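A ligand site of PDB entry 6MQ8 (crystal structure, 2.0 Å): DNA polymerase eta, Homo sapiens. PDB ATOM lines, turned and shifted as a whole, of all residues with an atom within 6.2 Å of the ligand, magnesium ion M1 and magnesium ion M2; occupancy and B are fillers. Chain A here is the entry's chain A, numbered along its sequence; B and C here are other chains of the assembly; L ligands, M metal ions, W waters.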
ATOM      1  N   ASP A  20      17.233 -16.785  -0.670  1.00  0.00           N
ATOM      2  CA  ASP A  20      17.198 -16.235  -2.025  1.00  0.00           C
ATOM      3  C   ASP A  20      17.668 -17.254  -3.049  1.00  0.00           C
ATOM      4  O   ASP A  20      18.778 -17.768  -2.965  1.00  0.00           O
ATOM      5  CB  ASP A  20      18.071 -14.990  -2.087  1.00  0.00           C
ATOM      6  CG  ASP A  20      17.942 -14.279  -3.424  1.00  0.00           C
ATOM      7  OD1 ASP A  20      18.585 -14.738  -4.386  1.00  0.00           O
ATOM      8  OD2 ASP A  20      17.180 -13.291  -3.519  1.00  0.00           O
ATOM      9  N   MET A  21      16.806 -17.570  -4.018  1.00  0.00           N
ATOM     10  CA  MET A  21      17.173 -18.562  -5.033  1.00  0.00           C
ATOM     11  C   MET A  21      18.367 -18.070  -5.847  1.00  0.00           C
ATOM     12  O   MET A  21      18.510 -16.870  -6.135  1.00  0.00           O
ATOM     13  CB  MET A  21      15.979 -18.827  -5.959  1.00  0.00           C
ATOM     14  CG  MET A  21      14.685 -19.100  -5.272  1.00  0.00           C
ATOM     15  SD  MET A  21      14.834 -20.445  -4.101  1.00  0.00           S
ATOM     16  CE  MET A  21      15.193 -21.808  -5.155  1.00  0.00           C
ATOM     17  N   ASP A  22      19.255 -19.005  -6.183  1.00  0.00           N
ATOM     18  CA  ASP A  22      20.410 -18.725  -7.031  1.00  0.00           C
ATOM     19  C   ASP A  22      19.962 -18.623  -8.472  1.00  0.00           C
ATOM     20  O   ASP A  22      19.233 -19.490  -8.959  1.00  0.00           O
ATOM     21  CB  ASP A  22      21.433 -19.837  -6.879  1.00  0.00           C
ATOM     22  CG  ASP A  22      22.020 -19.930  -5.453  1.00  0.00           C
ATOM     23  OD1 ASP A  22      21.965 -18.964  -4.715  1.00  0.00           O
ATOM     24  OD2 ASP A  22      22.537 -21.005  -5.066  1.00  0.00           O
ATOM     25  N   CYS A  23      20.445 -17.604  -9.160  1.00  0.00           N
ATOM     26  CA  CYS A  23      20.135 -17.302 -10.557  1.00  0.00           C
ATOM     27  C   CYS A  23      18.803 -17.862 -10.979  1.00  0.00           C
ATOM     28  O   CYS A  23      18.721 -18.717 -11.875  1.00  0.00           O
ATOM     29  CB  CYS A  23      21.253 -17.785 -11.489  1.00  0.00           C
ATOM     30  SG  CYS A  23      21.827 -19.485 -11.395  1.00  0.00           S
ATOM     31  N   PHE A  24      17.749 -17.386 -10.331  1.00  0.00           N
ATOM     32  CA  PHE A  24      16.475 -18.110 -10.276  1.00  0.00           C
ATOM     33  C   PHE A  24      15.879 -18.390 -11.653  1.00  0.00           C
ATOM     34  O   PHE A  24      15.534 -19.539 -11.973  1.00  0.00           O
ATOM     35  CB  PHE A  24      15.500 -17.297  -9.437  1.00  0.00           C
ATOM     36  CG  PHE A  24      14.172 -18.004  -9.210  1.00  0.00           C
ATOM     37  CD1 PHE A  24      14.124 -19.354  -8.888  1.00  0.00           C
ATOM     38  CD2 PHE A  24      12.992 -17.317  -9.382  1.00  0.00           C
ATOM     39  CE1 PHE A  24      12.927 -19.993  -8.688  1.00  0.00           C
ATOM     40  CE2 PHE A  24      11.773 -17.984  -9.168  1.00  0.00           C
ATOM     41  CZ  PHE A  24      11.769 -19.295  -8.833  1.00  0.00           C
ATOM     42  N   PHE A  25      15.732 -17.380 -12.489  1.00  0.00           N
ATOM     43  CA  PHE A  25      15.071 -17.647 -13.764  1.00  0.00           C
ATOM     44  C   PHE A  25      15.884 -18.613 -14.603  1.00  0.00           C
ATOM     45  O   PHE A  25      15.329 -19.409 -15.372  1.00  0.00           O
ATOM     46  CB  PHE A  25      14.827 -16.365 -14.561  1.00  0.00           C
ATOM     47  CG  PHE A  25      13.735 -15.473 -14.014  1.00  0.00           C
ATOM     48  CD1 PHE A  25      13.218 -15.652 -12.757  1.00  0.00           C
ATOM     49  CD2 PHE A  25      13.248 -14.431 -14.785  1.00  0.00           C
ATOM     50  CE1 PHE A  25      12.235 -14.838 -12.254  1.00  0.00           C
ATOM     51  CE2 PHE A  25      12.233 -13.583 -14.286  1.00  0.00           C
ATOM     52  CZ  PHE A  25      11.726 -13.787 -13.021  1.00  0.00           C
ATOM     53  N   VAL A  26      17.216 -18.590 -14.482  1.00  0.00           N
ATOM     54  CA  VAL A  26      18.047 -19.568 -15.178  1.00  0.00           C
ATOM     55  C   VAL A  26      17.786 -20.983 -14.647  1.00  0.00           C
ATOM     56  O   VAL A  26      17.603 -21.939 -15.426  1.00  0.00           O
ATOM     57  CB  VAL A  26      19.529 -19.177 -15.029  1.00  0.00           C
ATOM     58  CG1 VAL A  26      20.420 -20.310 -15.490  1.00  0.00           C
ATOM     59  CG2 VAL A  26      19.869 -17.929 -15.790  1.00  0.00           C
ATOM     60  N   ILE A  55      18.126 -10.747 -18.330  1.00  0.00           N
ATOM     61  CA  ILE A  55      17.603 -10.486 -16.989  1.00  0.00           C
ATOM     62  C   ILE A  55      18.068 -11.485 -15.945  1.00  0.00           C
ATOM     63  O   ILE A  55      17.872 -11.217 -14.743  1.00  0.00           O
ATOM     64  CB  ILE A  55      16.065 -10.396 -16.972  1.00  0.00           C
ATOM     65  CG1 ILE A  55      15.455 -11.669 -17.511  1.00  0.00           C
ATOM     66  CG2 ILE A  55      15.589  -9.169 -17.801  1.00  0.00           C
ATOM     67  CD1 ILE A  55      13.900 -11.712 -17.290  1.00  0.00           C
ATOM     68  N   ALA A  56      18.688 -12.592 -16.323  1.00  0.00           N
ATOM     69  CA  ALA A  56      19.257 -13.533 -15.367  1.00  0.00           C
ATOM     70  C   ALA A  56      20.439 -14.241 -15.995  1.00  0.00           C
ATOM     71  O   ALA A  56      20.423 -14.586 -17.175  1.00  0.00           O
ATOM     72  CB  ALA A  56      18.204 -14.550 -14.906  1.00  0.00           C
ATOM     73  N   VAL A  57      21.415 -14.566 -15.165  1.00  0.00           N
ATOM     74  CA  VAL A  57      22.715 -15.032 -15.636  1.00  0.00           C
ATOM     75  C   VAL A  57      23.194 -16.157 -14.734  1.00  0.00           C
ATOM     76  O   VAL A  57      23.293 -15.998 -13.513  1.00  0.00           O
ATOM     77  CB  VAL A  57      23.740 -13.873 -15.661  1.00  0.00           C
ATOM     78  CG1 VAL A  57      25.051 -14.300 -16.343  1.00  0.00           C
ATOM     79  CG2 VAL A  57      23.128 -12.631 -16.345  1.00  0.00           C
ATOM     80  N   TYR A  59      25.968 -18.689 -12.997  1.00  0.00           N
ATOM     81  CA  TYR A  59      27.261 -18.318 -12.393  1.00  0.00           C
ATOM     82  C   TYR A  59      28.415 -18.659 -13.329  1.00  0.00           C
ATOM     83  O   TYR A  59      29.438 -17.978 -13.314  1.00  0.00           O
ATOM     84  CB  TYR A  59      27.413 -19.009 -11.026  1.00  0.00           C
ATOM     85  CG  TYR A  59      26.666 -18.275  -9.948  1.00  0.00           C
ATOM     86  CD1 TYR A  59      25.292 -18.425  -9.800  1.00  0.00           C
ATOM     87  CD2 TYR A  59      27.327 -17.369  -9.126  1.00  0.00           C
ATOM     88  CE1 TYR A  59      24.610 -17.732  -8.860  1.00  0.00           C
ATOM     89  CE2 TYR A  59      26.649 -16.652  -8.191  1.00  0.00           C
ATOM     90  CZ  TYR A  59      25.280 -16.834  -8.046  1.00  0.00           C
ATOM     91  OH  TYR A  59      24.579 -16.090  -7.101  1.00  0.00           O
ATOM     92  N   ARG A  62      28.452 -15.568 -15.445  1.00  0.00           N
ATOM     93  CA  ARG A  62      28.945 -14.398 -14.730  1.00  0.00           C
ATOM     94  C   ARG A  62      30.473 -14.312 -14.760  1.00  0.00           C
ATOM     95  O   ARG A  62      31.033 -13.201 -14.800  1.00  0.00           O
ATOM     96  CB  ARG A  62      28.468 -14.389 -13.292  1.00  0.00           C
ATOM     97  CG  ARG A  62      26.945 -14.259 -13.183  1.00  0.00           C
ATOM     98  CD  ARG A  62      26.488 -14.291 -11.722  1.00  0.00           C
ATOM     99  NE  ARG A  62      25.061 -14.548 -11.633  1.00  0.00           N
ATOM    100  CZ  ARG A  62      24.315 -14.365 -10.544  1.00  0.00           C
ATOM    101  NH1 ARG A  62      24.859 -13.939  -9.434  1.00  0.00           N
ATOM    102  NH2 ARG A  62      23.028 -14.641 -10.593  1.00  0.00           N
ATOM    103  N   ARG A  68      23.160  -8.743 -15.880  1.00  0.00           N
ATOM    104  CA  ARG A  68      21.805  -8.267 -16.127  1.00  0.00           C
ATOM    105  C   ARG A  68      21.807  -6.927 -16.864  1.00  0.00           C
ATOM    106  O   ARG A  68      22.694  -6.097 -16.690  1.00  0.00           O
ATOM    107  CB  ARG A  68      21.056  -8.139 -14.815  1.00  0.00           C
ATOM    108  CG  ARG A  68      19.639  -7.571 -14.943  1.00  0.00           C
ATOM    109  CD  ARG A  68      18.885  -7.660 -13.599  1.00  0.00           C
ATOM    110  NE  ARG A  68      18.761  -9.040 -13.123  1.00  0.00           N
ATOM    111  CZ  ARG A  68      19.519  -9.572 -12.159  1.00  0.00           C
ATOM    112  NH1 ARG A  68      20.443  -8.828 -11.540  1.00  0.00           N
ATOM    113  NH2 ARG A  68      19.317 -10.847 -11.817  1.00  0.00           N
ATOM    114  N   SER A 120      10.177 -10.953  -2.753  1.00  0.00           N
ATOM    115  CA  SER A 120      10.323 -10.815  -4.199  1.00  0.00           C
ATOM    116  C   SER A 120       9.876 -12.132  -4.838  1.00  0.00           C
ATOM    117  O   SER A 120       9.453 -13.072  -4.156  1.00  0.00           O
ATOM    118  CB  SER A 120      11.766 -10.503  -4.594  1.00  0.00           C
ATOM    119  OG  SER A 120      12.604 -11.669  -4.561  1.00  0.00           O
ATOM    120  N   ILE A 121       9.978 -12.202  -6.166  1.00  0.00           N
ATOM    121  CA  ILE A 121       9.668 -13.464  -6.828  1.00  0.00           C
ATOM    122  C   ILE A 121      10.605 -14.609  -6.431  1.00  0.00           C
ATOM    123  O   ILE A 121      10.248 -15.790  -6.560  1.00  0.00           O
ATOM    124  CB  ILE A 121       9.685 -13.268  -8.347  1.00  0.00           C
ATOM    125  CG1 ILE A 121       8.904 -14.377  -9.042  1.00  0.00           C
ATOM    126  CG2 ILE A 121      11.107 -13.281  -8.901  1.00  0.00           C
ATOM    127  CD1 ILE A 121       8.663 -14.052 -10.519  1.00  0.00           C
ATOM    128  N   ASP A 122      11.787 -14.308  -5.874  1.00  0.00           N
ATOM    129  CA  ASP A 122      12.728 -15.383  -5.574  1.00  0.00           C
ATOM    130  C   ASP A 122      13.310 -15.358  -4.175  1.00  0.00           C
ATOM    131  O   ASP A 122      14.309 -16.044  -3.933  1.00  0.00           O
ATOM    132  CB  ASP A 122      13.882 -15.373  -6.585  1.00  0.00           C
ATOM    133  CG  ASP A 122      15.118 -14.632  -6.051  1.00  0.00           C
ATOM    134  OD1 ASP A 122      14.962 -13.498  -5.555  1.00  0.00           O
ATOM    135  OD2 ASP A 122      16.233 -15.181  -6.154  1.00  0.00           O
ATOM    136  N   GLU A 123      12.721 -14.620  -3.236  1.00  0.00           N
ATOM    137  CA  GLU A 123      13.231 -14.624  -1.879  1.00  0.00           C
ATOM    138  C   GLU A 123      12.146 -14.295  -0.879  1.00  0.00           C
ATOM    139  O   GLU A 123      11.164 -13.617  -1.183  1.00  0.00           O
ATOM    140  CB  GLU A 123      14.392 -13.644  -1.686  1.00  0.00           C
ATOM    141  CG  GLU A 123      14.021 -12.191  -1.688  1.00  0.00           C
ATOM    142  CD  GLU A 123      15.079 -11.340  -2.300  1.00  0.00           C
ATOM    143  OE1 GLU A 123      15.827 -10.682  -1.525  1.00  0.00           O
ATOM    144  OE2 GLU A 123      15.180 -11.306  -3.539  1.00  0.00           O
ATOM    145  N   SER A 220      20.593 -19.802  -1.675  1.00  0.00           N
ATOM    146  CA  SER A 220      21.454 -19.370  -0.589  1.00  0.00           C
ATOM    147  C   SER A 220      20.596 -18.763   0.506  1.00  0.00           C
ATOM    148  O   SER A 220      19.422 -18.449   0.299  1.00  0.00           O
ATOM    149  CB  SER A 220      22.498 -18.385  -1.105  1.00  0.00           C
ATOM    150  OG  SER A 220      23.260 -19.032  -2.159  1.00  0.00           O
ATOM    151  N   LYS A 231      19.669 -10.463   4.940  1.00  0.00           N
ATOM    152  CA  LYS A 231      19.852 -10.201   3.507  1.00  0.00           C
ATOM    153  C   LYS A 231      21.337 -10.042   3.152  1.00  0.00           C
ATOM    154  O   LYS A 231      21.807 -10.604   2.166  1.00  0.00           O
ATOM    155  CB  LYS A 231      19.064  -8.947   3.113  1.00  0.00           C
ATOM    156  CG  LYS A 231      19.245  -8.468   1.703  1.00  0.00           C
ATOM    157  CD  LYS A 231      18.659  -9.461   0.696  1.00  0.00           C
ATOM    158  CE  LYS A 231      18.810  -8.918  -0.746  1.00  0.00           C
ATOM    159  NZ  LYS A 231      18.377  -9.947  -1.735  1.00  0.00           N
ATOM    160  N   LYS A 238      27.053 -16.794  -1.698  1.00  0.00           N
ATOM    161  CA  LYS A 238      26.358 -17.332  -2.860  1.00  0.00           C
ATOM    162  C   LYS A 238      27.378 -17.868  -3.852  1.00  0.00           C
ATOM    163  O   LYS A 238      28.453 -17.302  -4.009  1.00  0.00           O
ATOM    164  CB  LYS A 238      25.536 -16.223  -3.544  1.00  0.00           C
ATOM    165  CG  LYS A 238      24.109 -16.172  -3.144  1.00  0.00           C
ATOM    166  CD  LYS A 238      23.339 -15.110  -3.925  1.00  0.00           C
ATOM    167  CE  LYS A 238      21.854 -15.174  -3.619  1.00  0.00           C
ATOM    168  NZ  LYS A 238      21.156 -16.271  -4.394  1.00  0.00           N
ATOM    169  N   PRO A 239      27.046 -18.923  -4.606  1.00  0.00           N
ATOM    170  CA  PRO A 239      25.782 -19.692  -4.573  1.00  0.00           C
ATOM    171  C   PRO A 239      25.794 -20.954  -3.730  1.00  0.00           C
ATOM    172  O   PRO A 239      26.842 -21.411  -3.357  1.00  0.00           O
ATOM    173  CB  PRO A 239      25.584 -20.071  -6.062  1.00  0.00           C
ATOM    174  CG  PRO A 239      27.035 -20.348  -6.514  1.00  0.00           C
ATOM    175  CD  PRO A 239      27.892 -19.319  -5.748  1.00  0.00           C
ATOM    176  P    DT B   8      16.333  -6.352  -2.581  1.00  0.00           P
ATOM    177  OP1  DT B   8      15.827  -7.079  -1.404  1.00  0.00           O
ATOM    178  OP2  DT B   8      17.742  -5.890  -2.729  1.00  0.00           O
ATOM    179  O5'  DT B   8      15.993  -7.219  -3.928  1.00  0.00           O
ATOM    180  C5'  DT B   8      14.796  -7.938  -3.990  1.00  0.00           C
ATOM    181  C4'  DT B   8      14.551  -8.463  -5.409  1.00  0.00           C
ATOM    182  O4'  DT B   8      14.138  -7.413  -6.281  1.00  0.00           O
ATOM    183  C3'  DT B   8      15.783  -9.088  -6.084  1.00  0.00           C
ATOM    184  O3'  DT B   8      15.554 -10.558  -6.153  1.00  0.00           O
ATOM    185  C2'  DT B   8      15.914  -8.428  -7.493  1.00  0.00           C
ATOM    186  C1'  DT B   8      14.555  -7.717  -7.626  1.00  0.00           C
ATOM    187  N1   DT B   8      14.555  -6.503  -8.397  1.00  0.00           N
ATOM    188  C2   DT B   8      13.620  -6.374  -9.411  1.00  0.00           C
ATOM    189  O2   DT B   8      12.776  -7.226  -9.667  1.00  0.00           O
ATOM    190  N3   DT B   8      13.688  -5.215 -10.095  1.00  0.00           N
ATOM    191  C4   DT B   8      14.579  -4.197  -9.877  1.00  0.00           C
ATOM    192  O4   DT B   8      14.585  -3.194 -10.548  1.00  0.00           O
ATOM    193  C5   DT B   8      15.513  -4.403  -8.831  1.00  0.00           C
ATOM    194  C7   DT B   8      16.523  -3.354  -8.524  1.00  0.00           C
ATOM    195  C6   DT B   8      15.472  -5.539  -8.153  1.00  0.00           C
ATOM    196  P    DI C   4      14.371  -0.812 -20.629  1.00  0.00           P
ATOM    197  OP1  DI C   4      14.612  -0.197 -21.974  1.00  0.00           O
ATOM    198  OP2  DI C   4      13.954   0.143 -19.550  1.00  0.00           O
ATOM    199  O5'  DI C   4      13.265  -2.043 -20.753  1.00  0.00           O
ATOM    200  C5'  DI C   4      13.394  -3.021 -21.735  1.00  0.00           C
ATOM    201  C4'  DI C   4      12.460  -4.217 -21.387  1.00  0.00           C
ATOM    202  O4'  DI C   4      12.898  -4.872 -20.318  1.00  0.00           O
ATOM    203  C3'  DI C   4      11.016  -3.769 -20.960  1.00  0.00           C
ATOM    204  O3'  DI C   4      10.166  -4.808 -21.149  1.00  0.00           O
ATOM    205  C2'  DI C   4      11.183  -3.450 -19.512  1.00  0.00           C
ATOM    206  C1'  DI C   4      11.968  -4.450 -19.081  1.00  0.00           C
ATOM    207  N9   DI C   4      12.842  -4.107 -17.987  1.00  0.00           N
ATOM    208  C8   DI C   4      13.505  -2.933 -17.771  1.00  0.00           C
ATOM    209  N7   DI C   4      14.206  -3.070 -16.613  1.00  0.00           N
ATOM    210  C5   DI C   4      14.005  -4.284 -16.151  1.00  0.00           C
ATOM    211  C6   DI C   4      14.522  -5.042 -14.924  1.00  0.00           C
ATOM    212  O6   DI C   4      15.267  -4.597 -14.155  1.00  0.00           O
ATOM    213  N1   DI C   4      14.126  -6.392 -14.705  1.00  0.00           N
ATOM    214  C2   DI C   4      13.245  -7.047 -15.632  1.00  0.00           C
ATOM    215  N3   DI C   4      12.766  -6.314 -16.793  1.00  0.00           N
ATOM    216  C4   DI C   4      13.179  -4.923 -17.007  1.00  0.00           C
ATOM    217  P    DA C   5       8.594  -4.653 -20.832  1.00  0.00           P
ATOM    218  OP1  DA C   5       7.927  -5.400 -21.894  1.00  0.00           O
ATOM    219  OP2  DA C   5       8.270  -3.209 -20.560  1.00  0.00           O
ATOM    220  O5'  DA C   5       8.426  -5.419 -19.453  1.00  0.00           O
ATOM    221  C5'  DA C   5       8.520  -6.844 -19.401  1.00  0.00           C
ATOM    222  C4'  DA C   5       8.273  -7.353 -18.000  1.00  0.00           C
ATOM    223  O4'  DA C   5       9.308  -6.887 -17.076  1.00  0.00           O
ATOM    224  C3'  DA C   5       6.936  -6.895 -17.401  1.00  0.00           C
ATOM    225  O3'  DA C   5       6.333  -7.985 -16.755  1.00  0.00           O
ATOM    226  C2'  DA C   5       7.304  -5.780 -16.414  1.00  0.00           C
ATOM    227  C1'  DA C   5       8.697  -6.279 -15.942  1.00  0.00           C
ATOM    228  N9   DA C   5       9.561  -5.264 -15.416  1.00  0.00           N
ATOM    229  C8   DA C   5       9.792  -4.021 -15.921  1.00  0.00           C
ATOM    230  N7   DA C   5      10.666  -3.331 -15.220  1.00  0.00           N
ATOM    231  C5   DA C   5      11.011  -4.193 -14.176  1.00  0.00           C
ATOM    232  C6   DA C   5      11.868  -4.043 -13.084  1.00  0.00           C
ATOM    233  N6   DA C   5      12.591  -2.922 -12.839  1.00  0.00           N
ATOM    234  N1   DA C   5      11.994  -5.099 -12.242  1.00  0.00           N
ATOM    235  C2   DA C   5      11.323  -6.199 -12.486  1.00  0.00           C
ATOM    236  N3   DA C   5      10.468  -6.450 -13.483  1.00  0.00           N
ATOM    237  C4   DA C   5      10.355  -5.385 -14.293  1.00  0.00           C
HETATM  238  P1  LIG L   1      21.371 -14.530  -7.442  1.00  0.00           P
HETATM  239  O1  LIG L   1      21.991 -15.902  -7.250  1.00  0.00           O
HETATM  240  O2  LIG L   1      20.266 -14.305  -6.481  1.00  0.00           O
HETATM  241  O3  LIG L   1      22.435 -13.463  -7.451  1.00  0.00           O
HETATM  242  P2  LIG L   1      19.211 -14.106  -9.249  1.00  0.00           P
HETATM  243  O4  LIG L   1      18.974 -14.347 -10.736  1.00  0.00           O
HETATM  244  O5  LIG L   1      18.284 -14.942  -8.392  1.00  0.00           O
HETATM  245  O6  LIG L   1      20.770 -14.478  -8.983  1.00  0.00           O
HETATM  246  P3  LIG L   1      17.814 -11.899  -7.880  1.00  0.00           P
HETATM  247  O7  LIG L   1      17.690 -12.801  -6.675  1.00  0.00           O
HETATM  248  O8  LIG L   1      18.175 -10.499  -7.513  1.00  0.00           O
HETATM  249  N1  LIG L   1      19.027 -12.469  -8.912  1.00  0.00           N
HETATM  250  O9  LIG L   1      16.350 -11.840  -8.685  1.00  0.00           O
HETATM  251  C1  LIG L   1      15.638 -13.105  -8.809  1.00  0.00           C
HETATM  252  C2  LIG L   1      15.056 -13.151 -10.264  1.00  0.00           C
HETATM  253  O10 LIG L   1      14.399 -12.045 -10.438  1.00  0.00           O
HETATM  254  C3  LIG L   1      16.192 -13.175 -11.326  1.00  0.00           C
HETATM  255  O11 LIG L   1      16.553 -14.457 -11.680  1.00  0.00           O
HETATM  256  C4  LIG L   1      15.576 -12.459 -12.450  1.00  0.00           C
HETATM  257  C5  LIG L   1      14.669 -11.622 -11.921  1.00  0.00           C
HETATM  258  N2  LIG L   1      15.181 -10.258 -11.813  1.00  0.00           N
HETATM  259  C6  LIG L   1      14.717  -9.237 -12.776  1.00  0.00           C
HETATM  260  N3  LIG L   1      15.251  -7.871 -12.644  1.00  0.00           N
HETATM  261  C7  LIG L   1      16.228  -7.509 -11.676  1.00  0.00           C
HETATM  262  C8  LIG L   1      16.705  -8.532 -10.734  1.00  0.00           C
HETATM  263  C9  LIG L   1      16.172  -9.905 -10.820  1.00  0.00           C
HETATM  264  O12 LIG L   1      13.915  -9.538 -13.641  1.00  0.00           O
HETATM  265  N4  LIG L   1      16.724  -6.147 -11.645  1.00  0.00           N
HETATM  266 MG    MG M   1      18.198 -14.754  -6.346  1.00  0.00          MG
HETATM  267 MG    MG M   2      16.444 -12.130  -4.964  1.00  0.00          MG
HETATM  268  O   HOH W   1      20.973 -13.570 -12.594  1.00  0.00           O
HETATM  269  O   HOH W   2      18.126 -10.782  -4.754  1.00  0.00           O
HETATM  270  O   HOH W   3      25.344 -13.267  -6.041  1.00  0.00           O
HETATM  271  O   HOH W   4      22.448 -11.367  -8.725  1.00  0.00           O
HETATM  272  O   HOH W   5      11.461 -10.373 -14.328  1.00  0.00           O
HETATM  273  O   HOH W   6      18.765  -5.714 -10.090  1.00  0.00           O
HETATM  274  O   HOH W   7      20.514 -12.411  -4.692  1.00  0.00           O
HETATM  275  O   HOH W   8      13.458 -10.849  -8.049  1.00  0.00           O
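Merely in contact with the ligand: Asp 22 (3.2 Å), Ile 55 (3.5 Å), Ala 56 (3.6 Å) and Ile 121 (3.8 Å).
16 residues have an atom within 4 Å of the ligand: Asp 20, Met 21, Asp 22, Cys 23, Phe 24, Phe 25, Ile 55, Ala 56, Tyr 59, Arg 62, Arg 68, Ile 121, Asp 122, Lys 238, DT 8 of chain B and DI 4 of chain C.
The nearest printed residue that does not touch the ligand is DA 5 of chain C (4.3 Å).
The side-chain hydroxyl (OH) of Tyr 59 sits at hydrogen-bond distance from an oxygen (O1) of the ligand (2.6 Å).
O6 of DI 4 of chain C lies within hydrogen-bond range of a nitrogen (N4) of the ligand (3.3 Å).
The guanidinium group of Arg 62 lies within salt-bridge range of an oxygen (O3) of the ligand, at 3.2 Å.
The backbone NH of Cys 23 is in hydrogen-bond range of an oxygen (O1) of the ligand.
An oxygen (O1) of the ligand is in salt-bridge range of the side-chain amino group of Lys 238, 3.0 Å away.
The backbone NH (N) of Phe 25 is in hydrogen-bond range of an oxygen (O11) of the ligand (3.1 Å).
The backbone NH (N) of Phe 24 is in hydrogen-bond range of an oxygen (O4) of the ligand (3.3 Å).
O4 of the ligand lies within salt-bridge range of NH2 of Arg 68.
Ser 120 touches magnesium ion M2 (OG to MG, 3.9 Å).
Of the 24 residues printed, 5 come within 4 Å of magnesium ion M2.
Magnesium ion M1 is bound by OD1 of Asp 20, at 2.0 Å.
Magnesium ion M1 is bound by OD2 of Asp 122 (2.0 Å).
Magnesium ion M1 is bound by an oxygen (O7) of the ligand (2.0 Å).
O5 of the ligand is bound to magnesium ion M1.
O2 of the ligand is bound to magnesium ion M1 (2.1 Å).
Magnesium ion M1 is bound by O of Met 21, at 2.1 Å.
The backbone carbonyl oxygen of Asp 20 sits at hydrogen-bond distance from the side-chain amino group of Lys 238, 3.2 Å away.
The side-chain amino group (NZ) of Lys 231 sits close to the side-chain carboxylate (OD2) of Asp 20 (3.97 Å).
N of Glu 123 sits at hydrogen-bond distance from OG of Ser 120 (3.2 Å).
OE1 of Glu 123 lies within salt-bridge range of NZ of Lys 231, 2.7 Å away.
The backbone carbonyl oxygen of Met 21 lies close to the side-chain amino group of Lys 238 (3.2 Å).
N1 of DA 5 of chain C lies close to N3 of DT 8 of chain B.
NZ of Lys 231 is in salt-bridge range of OP1 of DT 8 of chain B, 3.9 Å away.
The side-chain carboxylate (OD1) of Asp 22 lies within hydrogen-bond range of the side-chain hydroxyl (OG) of Ser 220, 2.9 Å away.
Merely in contact with magnesium ion M1: Lys 238 (3.9 Å).
Within 4 Å of magnesium ion M1: Asp 20, Met 21, Asp 122 and Lys 238.
The nearest printed residue that does not touch magnesium ion M1 is Asp 22 (4.4 Å).
Magnesium ion M2 is bound by the side-chain carboxylate of Asp 20 (2.0 Å), the side-chain carboxylate of Glu 123 (2.1 Å), the side-chain carboxylate of Asp 122 (2.1 Å), O3' of DT 8 of chain B (2.2 Å), water W2 (2.2 Å) and an oxygen (O7) of the ligand (2.2 Å).
Magnesium ion M2 has six donor atoms within binding distance.
Water W2 lies within hydrogen-bond range of an oxygen (O8) of the ligand (2.8 Å) and the side-chain amino group (NZ) of Lys 231 (3.1 Å).
Water W3 lies within hydrogen-bond range of OH of Tyr 59, O3 of the ligand and NH1 of Arg 62.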
